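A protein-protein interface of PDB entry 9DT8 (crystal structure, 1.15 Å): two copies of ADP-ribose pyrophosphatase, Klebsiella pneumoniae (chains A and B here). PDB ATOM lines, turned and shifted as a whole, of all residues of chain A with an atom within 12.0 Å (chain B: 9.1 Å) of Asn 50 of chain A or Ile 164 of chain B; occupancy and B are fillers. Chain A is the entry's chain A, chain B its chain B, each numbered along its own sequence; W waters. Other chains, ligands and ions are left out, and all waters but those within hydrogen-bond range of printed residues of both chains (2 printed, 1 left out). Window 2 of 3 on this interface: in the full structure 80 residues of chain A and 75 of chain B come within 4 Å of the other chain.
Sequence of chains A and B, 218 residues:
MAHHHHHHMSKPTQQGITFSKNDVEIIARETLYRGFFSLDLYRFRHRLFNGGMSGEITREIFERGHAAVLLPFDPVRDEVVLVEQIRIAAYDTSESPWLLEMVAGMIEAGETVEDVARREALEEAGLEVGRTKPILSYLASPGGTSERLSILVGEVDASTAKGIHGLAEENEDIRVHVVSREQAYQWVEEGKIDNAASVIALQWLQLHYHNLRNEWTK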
ATOM      1  N   GLY A  16     -15.821  22.341  27.244  1.00  0.00           N
ATOM      2  CA  GLY A  16     -14.791  21.607  27.943  1.00  0.00           C
ATOM      3  C   GLY A  16     -14.964  20.111  27.792  1.00  0.00           C
ATOM      4  O   GLY A  16     -15.391  19.632  26.736  1.00  0.00           O
ATOM      5  N   ILE A  17     -14.662  19.361  28.855  1.00  0.00           N
ATOM      6  CA  ILE A  17     -14.643  17.912  28.754  1.00  0.00           C
ATOM      7  C   ILE A  17     -16.058  17.355  28.644  1.00  0.00           C
ATOM      8  O   ILE A  17     -17.056  17.954  29.066  1.00  0.00           O
ATOM      9  CB  ILE A  17     -13.877  17.246  29.908  1.00  0.00           C
ATOM     10  CG1 ILE A  17     -14.581  17.541  31.230  1.00  0.00           C
ATOM     11  CG2 ILE A  17     -12.378  17.669  29.911  1.00  0.00           C
ATOM     12  CD1 ILE A  17     -14.045  16.725  32.363  1.00  0.00           C
ATOM     13  N   THR A  18     -16.120  16.141  28.122  1.00  0.00           N
ATOM     14  CA  THR A  18     -17.350  15.530  27.657  1.00  0.00           C
ATOM     15  C   THR A  18     -17.978  14.603  28.678  1.00  0.00           C
ATOM     16  O   THR A  18     -19.205  14.518  28.751  1.00  0.00           O
ATOM     17  CB  THR A  18     -17.018  14.738  26.386  1.00  0.00           C
ATOM     18  OG1 THR A  18     -16.388  15.607  25.438  1.00  0.00           O
ATOM     19  CG2 THR A  18     -18.249  14.135  25.770  1.00  0.00           C
ATOM     20  N   PHE A  19     -17.167  13.923  29.467  1.00  0.00           N
ATOM     21  CA  PHE A  19     -17.618  12.826  30.303  1.00  0.00           C
ATOM     22  C   PHE A  19     -17.114  13.020  31.726  1.00  0.00           C
ATOM     23  O   PHE A  19     -16.105  13.694  31.967  1.00  0.00           O
ATOM     24  CB  PHE A  19     -17.118  11.481  29.756  1.00  0.00           C
ATOM     25  CG  PHE A  19     -17.731  11.076  28.426  1.00  0.00           C
ATOM     26  CD1 PHE A  19     -19.098  10.924  28.275  1.00  0.00           C
ATOM     27  CD2 PHE A  19     -16.923  10.809  27.333  1.00  0.00           C
ATOM     28  CE1 PHE A  19     -19.637  10.544  27.063  1.00  0.00           C
ATOM     29  CE2 PHE A  19     -17.466  10.419  26.128  1.00  0.00           C
ATOM     30  CZ  PHE A  19     -18.823  10.291  25.992  1.00  0.00           C
ATOM     31  N   ASP A  23     -19.399   8.085  33.826  1.00  0.00           N
ATOM     32  CA  ASP A  23     -19.206   7.516  32.502  1.00  0.00           C
ATOM     33  C   ASP A  23     -18.078   6.504  32.438  1.00  0.00           C
ATOM     34  O   ASP A  23     -17.770   6.009  31.352  1.00  0.00           O
ATOM     35  CB  ASP A  23     -18.956   8.653  31.522  1.00  0.00           C
ATOM     36  CG  ASP A  23     -20.131   9.585  31.444  1.00  0.00           C
ATOM     37  OD1 ASP A  23     -21.254   9.079  31.249  1.00  0.00           O
ATOM     38  OD2 ASP A  23     -19.956  10.810  31.613  1.00  0.00           O
ATOM     39  N   HIS A  46     -15.184   2.401  29.770  1.00  0.00           N
ATOM     40  CA  HIS A  46     -15.557   3.809  29.757  1.00  0.00           C
ATOM     41  C   HIS A  46     -16.383   4.124  28.520  1.00  0.00           C
ATOM     42  O   HIS A  46     -16.292   3.450  27.486  1.00  0.00           O
ATOM     43  CB  HIS A  46     -14.311   4.718  29.828  1.00  0.00           C
ATOM     44  CG  HIS A  46     -13.407   4.582  28.648  1.00  0.00           C
ATOM     45  ND1 HIS A  46     -13.615   5.267  27.471  1.00  0.00           N
ATOM     46  CD2 HIS A  46     -12.300   3.830  28.455  1.00  0.00           C
ATOM     47  CE1 HIS A  46     -12.671   4.943  26.606  1.00  0.00           C
ATOM     48  NE2 HIS A  46     -11.858   4.077  27.182  1.00  0.00           N
ATOM     49  N   ARG A  47     -17.177   5.186  28.645  1.00  0.00           N
ATOM     50  CA  ARG A  47     -17.975   5.672  27.535  1.00  0.00           C
ATOM     51  C   ARG A  47     -17.075   6.132  26.399  1.00  0.00           C
ATOM     52  O   ARG A  47     -15.967   6.632  26.613  1.00  0.00           O
ATOM     53  CB  ARG A  47     -18.834   6.855  27.989  1.00  0.00           C
ATOM     54  CG  ARG A  47     -20.073   6.496  28.823  1.00  0.00           C
ATOM     55  CD  ARG A  47     -21.239   5.939  27.993  1.00  0.00           C
ATOM     56  NE  ARG A  47     -21.346   6.539  26.667  1.00  0.00           N
ATOM     57  CZ  ARG A  47     -21.995   7.664  26.386  1.00  0.00           C
ATOM     58  NH1 ARG A  47     -22.614   8.363  27.327  1.00  0.00           N
ATOM     59  NH2 ARG A  47     -22.018   8.100  25.130  1.00  0.00           N
ATOM     60  N   LEU A  48     -17.571   5.954  25.178  1.00  0.00           N
ATOM     61  CA  LEU A  48     -16.898   6.335  23.948  1.00  0.00           C
ATOM     62  C   LEU A  48     -17.578   7.560  23.353  1.00  0.00           C
ATOM     63  O   LEU A  48     -18.799   7.716  23.432  1.00  0.00           O
ATOM     64  CB  LEU A  48     -16.950   5.200  22.919  1.00  0.00           C
ATOM     65  CG  LEU A  48     -16.289   3.884  23.321  1.00  0.00           C
ATOM     66  CD1 LEU A  48     -16.596   2.791  22.281  1.00  0.00           C
ATOM     67  CD2 LEU A  48     -14.792   4.067  23.488  1.00  0.00           C
ATOM     68  N   PHE A  49     -16.778   8.423  22.723  1.00  0.00           N
ATOM     69  CA  PHE A  49     -17.321   9.665  22.184  1.00  0.00           C
ATOM     70  C   PHE A  49     -18.413   9.418  21.153  1.00  0.00           C
ATOM     71  O   PHE A  49     -19.363  10.202  21.063  1.00  0.00           O
ATOM     72  CB  PHE A  49     -16.211  10.508  21.565  1.00  0.00           C
ATOM     73  CG  PHE A  49     -15.248  11.048  22.572  1.00  0.00           C
ATOM     74  CD1 PHE A  49     -15.653  11.980  23.528  1.00  0.00           C
ATOM     75  CD2 PHE A  49     -13.931  10.639  22.575  1.00  0.00           C
ATOM     76  CE1 PHE A  49     -14.767  12.465  24.461  1.00  0.00           C
ATOM     77  CE2 PHE A  49     -13.038  11.123  23.509  1.00  0.00           C
ATOM     78  CZ  PHE A  49     -13.453  12.034  24.441  1.00  0.00           C
ATOM     79  N   ASN A  50     -18.275   8.367  20.340  1.00  0.00           N
ATOM     80  CA  ASN A  50     -19.264   8.078  19.305  1.00  0.00           C
ATOM     81  C   ASN A  50     -20.447   7.276  19.838  1.00  0.00           C
ATOM     82  O   ASN A  50     -21.340   6.922  19.059  1.00  0.00           O
ATOM     83  CB  ASN A  50     -18.602   7.354  18.120  1.00  0.00           C
ATOM     84  CG  ASN A  50     -17.695   8.271  17.280  1.00  0.00           C
ATOM     85  OD1 ASN A  50     -18.088   9.372  16.884  1.00  0.00           O
ATOM     86  ND2 ASN A  50     -16.469   7.813  17.015  1.00  0.00           N
ATOM     87  N   GLY A  51     -20.493   7.005  21.129  1.00  0.00           N
ATOM     88  CA  GLY A  51     -21.576   6.253  21.723  1.00  0.00           C
ATOM     89  C   GLY A  51     -21.133   4.874  22.183  1.00  0.00           C
ATOM     90  O   GLY A  51     -20.222   4.251  21.614  1.00  0.00           O
ATOM     91  N   GLY A  52     -21.779   4.391  23.230  1.00  0.00           N
ATOM     92  CA  GLY A  52     -21.506   3.065  23.727  1.00  0.00           C
ATOM     93  C   GLY A  52     -20.327   3.060  24.668  1.00  0.00           C
ATOM     94  O   GLY A  52     -19.755   4.092  25.026  1.00  0.00           O
ATOM     95  N   MET A  53     -19.963   1.850  25.077  1.00  0.00           N
ATOM     96  CA  MET A  53     -18.935   1.612  26.072  1.00  0.00           C
ATOM     97  C   MET A  53     -17.780   0.848  25.447  1.00  0.00           C
ATOM     98  O   MET A  53     -17.975  -0.012  24.575  1.00  0.00           O
ATOM     99  CB  MET A  53     -19.487   0.774  27.238  1.00  0.00           C
ATOM    100  CG  MET A  53     -20.523   1.488  28.091  1.00  0.00           C
ATOM    101  SD  MET A  53     -19.884   2.891  29.013  1.00  0.00           S
ATOM    102  CE  MET A  53     -18.649   2.130  30.032  1.00  0.00           C
ATOM    103  N   SER A  54     -16.577   1.167  25.914  1.00  0.00           N
ATOM    104  CA  SER A  54     -15.397   0.415  25.541  1.00  0.00           C
ATOM    105  C   SER A  54     -15.478  -1.014  26.078  1.00  0.00           C
ATOM    106  O   SER A  54     -16.306  -1.346  26.931  1.00  0.00           O
ATOM    107  CB  SER A  54     -14.150   1.060  26.152  1.00  0.00           C
ATOM    108  OG  SER A  54     -14.090   0.853  27.560  1.00  0.00           O
ATOM    109  N   VAL B  83      -6.536  17.747  22.724  1.00  0.00           N
ATOM    110  CA  VAL B  83      -7.136  16.426  22.577  1.00  0.00           C
ATOM    111  C   VAL B  83      -7.665  15.984  23.933  1.00  0.00           C
ATOM    112  O   VAL B  83      -7.017  16.177  24.962  1.00  0.00           O
ATOM    113  CB  VAL B  83      -6.182  15.386  21.946  1.00  0.00           C
ATOM    114  CG1 VAL B  83      -5.917  15.720  20.481  1.00  0.00           C
ATOM    115  CG2 VAL B  83      -4.849  15.256  22.690  1.00  0.00           C
ATOM    116  N   GLU B  84      -8.853  15.412  23.935  1.00  0.00           N
ATOM    117  CA  GLU B  84      -9.515  14.930  25.137  1.00  0.00           C
ATOM    118  C   GLU B  84      -9.565  13.404  25.112  1.00  0.00           C
ATOM    119  O   GLU B  84     -10.029  12.792  24.145  1.00  0.00           O
ATOM    120  CB  GLU B  84     -10.940  15.493  25.244  1.00  0.00           C
ATOM    121  CG  GLU B  84     -11.660  15.055  26.501  1.00  0.00           C
ATOM    122  CD  GLU B  84     -13.169  15.281  26.485  1.00  0.00           C
ATOM    123  OE1 GLU B  84     -13.723  15.821  25.501  1.00  0.00           O
ATOM    124  OE2 GLU B  84     -13.787  14.899  27.500  1.00  0.00           O
ATOM    125  N   LEU B 122      -1.233  13.116  13.473  1.00  0.00           N
ATOM    126  CA  LEU B 122      -2.175  12.544  12.520  1.00  0.00           C
ATOM    127  C   LEU B 122      -3.097  11.534  13.197  1.00  0.00           C
ATOM    128  O   LEU B 122      -4.313  11.573  12.999  1.00  0.00           O
ATOM    129  CB  LEU B 122      -1.417  11.918  11.351  1.00  0.00           C
ATOM    130  CG  LEU B 122      -2.313  11.518  10.179  1.00  0.00           C
ATOM    131  CD1 LEU B 122      -2.892  12.735   9.464  1.00  0.00           C
ATOM    132  CD2 LEU B 122      -1.533  10.662   9.200  1.00  0.00           C
ATOM    133  N   GLU B 123      -2.538  10.647  14.030  1.00  0.00           N
ATOM    134  CA  GLU B 123      -3.327   9.579  14.650  1.00  0.00           C
ATOM    135  C   GLU B 123      -4.289  10.114  15.705  1.00  0.00           C
ATOM    136  O   GLU B 123      -5.405   9.601  15.842  1.00  0.00           O
ATOM    137  CB  GLU B 123      -2.417   8.511  15.276  1.00  0.00           C
ATOM    138  CG  GLU B 123      -1.473   7.815  14.314  1.00  0.00           C
ATOM    139  CD  GLU B 123      -0.589   6.740  14.965  1.00  0.00           C
ATOM    140  OE1 GLU B 123      -0.583   6.632  16.213  1.00  0.00           O
ATOM    141  OE2 GLU B 123       0.095   6.000  14.215  1.00  0.00           O
ATOM    142  N   GLU B 124      -3.868  11.115  16.481  1.00  0.00           N
ATOM    143  CA  GLU B 124      -4.665  11.598  17.599  1.00  0.00           C
ATOM    144  C   GLU B 124      -5.537  12.783  17.250  1.00  0.00           C
ATOM    145  O   GLU B 124      -6.533  13.010  17.935  1.00  0.00           O
ATOM    146  CB  GLU B 124      -3.757  11.982  18.776  1.00  0.00           C
ATOM    147  CG  GLU B 124      -2.937  10.795  19.257  1.00  0.00           C
ATOM    148  CD  GLU B 124      -2.190  11.012  20.553  1.00  0.00           C
ATOM    149  OE1 GLU B 124      -1.934  12.179  20.920  1.00  0.00           O
ATOM    150  OE2 GLU B 124      -1.836   9.995  21.212  1.00  0.00           O
ATOM    151  N   ALA B 125      -5.199  13.538  16.214  1.00  0.00           N
ATOM    152  CA  ALA B 125      -5.932  14.759  15.932  1.00  0.00           C
ATOM    153  C   ALA B 125      -6.233  14.959  14.458  1.00  0.00           C
ATOM    154  O   ALA B 125      -6.835  15.973  14.101  1.00  0.00           O
ATOM    155  CB  ALA B 125      -5.183  15.980  16.499  1.00  0.00           C
ATOM    156  N   GLY B 126      -5.826  14.042  13.591  1.00  0.00           N
ATOM    157  CA  GLY B 126      -6.077  14.199  12.171  1.00  0.00           C
ATOM    158  C   GLY B 126      -5.333  15.342  11.531  1.00  0.00           C
ATOM    159  O   GLY B 126      -5.763  15.835  10.484  1.00  0.00           O
ATOM    160  N   ALA B 161      -8.735  20.752  12.278  1.00  0.00           N
ATOM    161  CA  ALA B 161      -8.688  19.971  13.507  1.00  0.00           C
ATOM    162  C   ALA B 161     -10.108  19.801  14.001  1.00  0.00           C
ATOM    163  O   ALA B 161     -10.741  20.782  14.399  1.00  0.00           O
ATOM    164  CB  ALA B 161      -7.871  20.703  14.568  1.00  0.00           C
ATOM    165  N   LYS B 162     -10.613  18.575  13.975  1.00  0.00           N
ATOM    166  CA  LYS B 162     -11.974  18.327  14.423  1.00  0.00           C
ATOM    167  C   LYS B 162     -12.228  16.830  14.448  1.00  0.00           C
ATOM    168  O   LYS B 162     -11.564  16.054  13.756  1.00  0.00           O
ATOM    169  CB  LYS B 162     -13.002  19.005  13.509  1.00  0.00           C
ATOM    170  CG  LYS B 162     -13.021  18.458  12.097  1.00  0.00           C
ATOM    171  CD  LYS B 162     -13.571  19.474  11.100  1.00  0.00           C
ATOM    172  CE  LYS B 162     -12.542  19.801  10.035  1.00  0.00           C
ATOM    173  NZ  LYS B 162     -12.922  20.991   9.236  1.00  0.00           N
ATOM    174  N   GLY B 163     -13.198  16.447  15.251  1.00  0.00           N
ATOM    175  CA  GLY B 163     -13.680  15.084  15.246  1.00  0.00           C
ATOM    176  C   GLY B 163     -13.042  14.158  16.260  1.00  0.00           C
ATOM    177  O   GLY B 163     -12.324  14.551  17.184  1.00  0.00           O
ATOM    178  N   ILE B 164     -13.348  12.880  16.076  1.00  0.00           N
ATOM    179  CA  ILE B 164     -12.953  11.803  16.971  1.00  0.00           C
ATOM    180  C   ILE B 164     -11.872  10.973  16.288  1.00  0.00           C
ATOM    181  O   ILE B 164     -12.038  10.530  15.143  1.00  0.00           O
ATOM    182  CB  ILE B 164     -14.162  10.926  17.362  1.00  0.00           C
ATOM    183  CG1 ILE B 164     -15.288  11.763  17.974  1.00  0.00           C
ATOM    184  CG2 ILE B 164     -13.746   9.825  18.297  1.00  0.00           C
ATOM    185  CD1 ILE B 164     -14.873  12.684  19.083  1.00  0.00           C
ATOM    186  N   HIS B 165     -10.780  10.742  17.004  1.00  0.00           N
ATOM    187  CA  HIS B 165      -9.616  10.054  16.468  1.00  0.00           C
ATOM    188  C   HIS B 165      -9.160   8.976  17.433  1.00  0.00           C
ATOM    189  O   HIS B 165      -9.861   8.643  18.390  1.00  0.00           O
ATOM    190  CB  HIS B 165      -8.527  11.079  16.166  1.00  0.00           C
ATOM    191  CG  HIS B 165      -8.960  12.091  15.158  1.00  0.00           C
ATOM    192  ND1 HIS B 165      -8.730  11.948  13.806  1.00  0.00           N
ATOM    193  CD2 HIS B 165      -9.689  13.223  15.304  1.00  0.00           C
ATOM    194  CE1 HIS B 165      -9.263  12.977  13.169  1.00  0.00           C
ATOM    195  NE2 HIS B 165      -9.850  13.761  14.055  1.00  0.00           N
ATOM    196  N   GLY B 166      -7.985   8.423  17.192  1.00  0.00           N
ATOM    197  CA  GLY B 166      -7.502   7.301  17.963  1.00  0.00           C
ATOM    198  C   GLY B 166      -7.784   5.966  17.286  1.00  0.00           C
ATOM    199  O   GLY B 166      -8.577   5.856  16.347  1.00  0.00           O
ATOM    200  N   LEU B 167      -7.103   4.932  17.766  1.00  0.00           N
ATOM    201  CA  LEU B 167      -7.280   3.576  17.240  1.00  0.00           C
ATOM    202  C   LEU B 167      -8.418   2.852  17.956  1.00  0.00           C
ATOM    203  O   LEU B 167      -8.264   2.410  19.100  1.00  0.00           O
ATOM    204  CB  LEU B 167      -5.988   2.769  17.390  1.00  0.00           C
ATOM    205  N   GLU B 172      -8.360   3.237  22.194  1.00  0.00           N
ATOM    206  CA  GLU B 172      -8.002   4.657  22.117  1.00  0.00           C
ATOM    207  C   GLU B 172      -9.133   5.476  21.510  1.00  0.00           C
ATOM    208  O   GLU B 172      -9.538   5.241  20.368  1.00  0.00           O
ATOM    209  CB  GLU B 172      -6.727   4.817  21.282  1.00  0.00           C
ATOM    210  CG  GLU B 172      -6.073   6.162  21.434  1.00  0.00           C
ATOM    211  CD  GLU B 172      -4.748   6.250  20.700  1.00  0.00           C
ATOM    212  OE1 GLU B 172      -4.743   6.177  19.449  1.00  0.00           O
ATOM    213  OE2 GLU B 172      -3.711   6.381  21.381  1.00  0.00           O
ATOM    214  N   ASP B 173      -9.608   6.464  22.266  1.00  0.00           N
ATOM    215  CA  ASP B 173     -10.771   7.272  21.894  1.00  0.00           C
ATOM    216  C   ASP B 173     -10.471   8.718  22.274  1.00  0.00           C
ATOM    217  O   ASP B 173     -10.299   9.030  23.457  1.00  0.00           O
ATOM    218  CB  ASP B 173     -11.992   6.725  22.628  1.00  0.00           C
ATOM    219  CG  ASP B 173     -13.294   7.307  22.138  1.00  0.00           C
ATOM    220  OD1 ASP B 173     -13.489   7.434  20.911  1.00  0.00           O
ATOM    221  OD2 ASP B 173     -14.139   7.625  22.995  1.00  0.00           O
ATOM    222  N   ILE B 174     -10.376   9.589  21.268  1.00  0.00           N
ATOM    223  CA  ILE B 174      -9.803  10.919  21.435  1.00  0.00           C
ATOM    224  C   ILE B 174     -10.691  11.930  20.722  1.00  0.00           C
ATOM    225  O   ILE B 174     -10.988  11.770  19.535  1.00  0.00           O
ATOM    226  CB  ILE B 174      -8.366  10.982  20.870  1.00  0.00           C
ATOM    227  CG1 ILE B 174      -7.500   9.879  21.477  1.00  0.00           C
ATOM    228  CG2 ILE B 174      -7.752  12.358  21.111  1.00  0.00           C
ATOM    229  CD1 ILE B 174      -6.104   9.830  20.901  1.00  0.00           C
ATOM    230  N   ARG B 175     -11.077  12.990  21.421  1.00  0.00           N
ATOM    231  CA  ARG B 175     -11.886  14.057  20.852  1.00  0.00           C
ATOM    232  C   ARG B 175     -11.051  15.319  20.704  1.00  0.00           C
ATOM    233  O   ARG B 175     -10.416  15.761  21.665  1.00  0.00           O
ATOM    234  CB  ARG B 175     -13.113  14.325  21.730  1.00  0.00           C
ATOM    235  CG  ARG B 175     -13.976  15.455  21.218  1.00  0.00           C
ATOM    236  CD  ARG B 175     -15.229  15.614  22.068  1.00  0.00           C
ATOM    237  NE  ARG B 175     -16.114  16.622  21.504  1.00  0.00           N
ATOM    238  CZ  ARG B 175     -17.329  16.897  21.957  1.00  0.00           C
ATOM    239  NH1 ARG B 175     -17.821  16.287  23.018  1.00  0.00           N
ATOM    240  NH2 ARG B 175     -18.074  17.796  21.318  1.00  0.00           N
ATOM    241  N   VAL B 176     -11.093  15.920  19.532  1.00  0.00           N
ATOM    242  CA  VAL B 176     -10.372  17.161  19.281  1.00  0.00           C
ATOM    243  C   VAL B 176     -11.200  18.339  19.769  1.00  0.00           C
ATOM    244  O   VAL B 176     -12.406  18.420  19.515  1.00  0.00           O
ATOM    245  CB  VAL B 176     -10.073  17.284  17.772  1.00  0.00           C
ATOM    246  CG1 VAL B 176      -9.604  18.710  17.410  1.00  0.00           C
ATOM    247  CG2 VAL B 176      -9.060  16.244  17.341  1.00  0.00           C
ATOM    248  N   HIS B 177     -10.539  19.299  20.391  1.00  0.00           N
ATOM    249  CA  HIS B 177     -11.146  20.565  20.757  1.00  0.00           C
ATOM    250  C   HIS B 177     -10.250  21.674  20.235  1.00  0.00           C
ATOM    251  O   HIS B 177      -9.025  21.596  20.380  1.00  0.00           O
ATOM    252  CB  HIS B 177     -11.219  20.731  22.270  1.00  0.00           C
ATOM    253  CG  HIS B 177     -12.104  19.754  22.956  1.00  0.00           C
ATOM    254  ND1 HIS B 177     -13.385  20.063  23.351  1.00  0.00           N
ATOM    255  CD2 HIS B 177     -11.879  18.477  23.335  1.00  0.00           C
ATOM    256  CE1 HIS B 177     -13.915  19.007  23.941  1.00  0.00           C
ATOM    257  NE2 HIS B 177     -13.017  18.038  23.957  1.00  0.00           N
HETATM  258  O   HOH W   1     -15.872   6.875  19.882  1.00  0.00           O
HETATM  259  O   HOH W   2     -13.858   8.316  25.703  1.00  0.00           O
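The backbone NH of Phe 49 of chain A sits at hydrogen-bond distance from the side-chain carboxylate of Asp 173 of chain B (2.8 Å). The side-chain hydroxyl (OG1) of Thr 18 of chain A lies within hydrogen-bond range of the guanidinium group (NH1) of Arg 175 of chain B. The side-chain hydroxyl (OG1) of Thr 18 of chain A sits at hydrogen-bond distance from the side-chain carboxylate (OE1) of Glu 84 of chain B (2.7 Å).
The backbone NH (N) of Glu 84 of chain B sits at hydrogen-bond distance from the backbone carbonyl oxygen (O) of Arg 175 of chain B (2.8 Å). A ring nitrogen (NE2) of His 177 of chain B lies within hydrogen-bond range of the side-chain carboxylate (OE1) of Glu 84 of chain B (2.8 Å). The backbone NH of His 165 of chain B lies within hydrogen-bond range of the backbone carbonyl oxygen of Ile 174 of chain B.
Among the printed residues, merely in contact across the chains: Leu 48 of chain A with Asp 173 of chain B, Gly 16 of chain A with His 177 of chain B, Ile 17 of chain A with Glu 84 of chain B, Phe 49 of chain A with Arg 175 of chain B, Phe 49 of chain A with Glu 84 of chain B, Phe 49 of chain A with Ile 164 of chain B, Asn 50 of chain A with Ile 164 of chain B and Phe 49 of chain A with Ile 174 of chain B.
Printed residues of chain B within 4 Å of Ile 17 of chain A: Glu 84. Printed residues of chain B within 4 Å of Thr 18 of chain A: Glu 84 (2.7 Å) and Arg 175 (2.9 Å). Printed residues of chain B within 4 Å of Phe 49 of chain A: Glu 84, Ile 164, Asp 173, Ile 174 and Arg 175. Of chain B, only Ile 164 (3.6 Å) comes within 4 Å of Asn 50 of chain A. Of the printed residues of chain A, Glu 84 of chain B touches Ile 17 (3.4 Å), Thr 18 (2.7 Å) and Phe 49 (3.5 Å). Glu 124 of chain B touches none of the printed residues of chain A. No residue of chain A comes within 4 Å of Gly 163 of chain B. Printed residues of chain A within 4 Å of Ile 164 of chain B: Phe 49 and Asn 50. No residue of chain A comes within 4 Å of His 165 of chain B. Of chain A, only Phe 49 comes within 4 Å of Ile 174 of chain B. No residue of chain A comes within 4 Å of Val 176 of chain B. Printed residues of chain A within 4 Å of His 177 of chain B: Gly 16 (3.2 Å). The nearest residue of chain B that does not touch Asn 50 of chain A is Asp 173 of chain B (4.9 Å).
Hydrophobic or aromatic side chains of chain B that line the printed part of chain A: Ile 164 and His 177. Of the 14 printed residues of chain A, 6 touch a printed residue of chain B. Printed residues of chain A that touch a printed residue of chain B: Gly 16, Ile 17, Thr 18, Leu 48, Phe 49 and Asn 50. Among the printed residues, no Asp or Glu carboxylate lies within 4 Å of a Lys or Arg side-chain nitrogen of the other chain.
No position is printed for both chains. Of the 11 pairs that touch across the chains among the printed residues, none has its exchanged pair printed and touching as well.
Water W1 lies within hydrogen-bond range of OD1 of Asp 173 of chain B, N of Asn 50 of chain A and N of Phe 49 of chain A. Water W2 lies within hydrogen-bond range of OD2 of Asp 173 of chain B (2.8 Å) and O of Arg 47 of chain A (2.8 Å).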
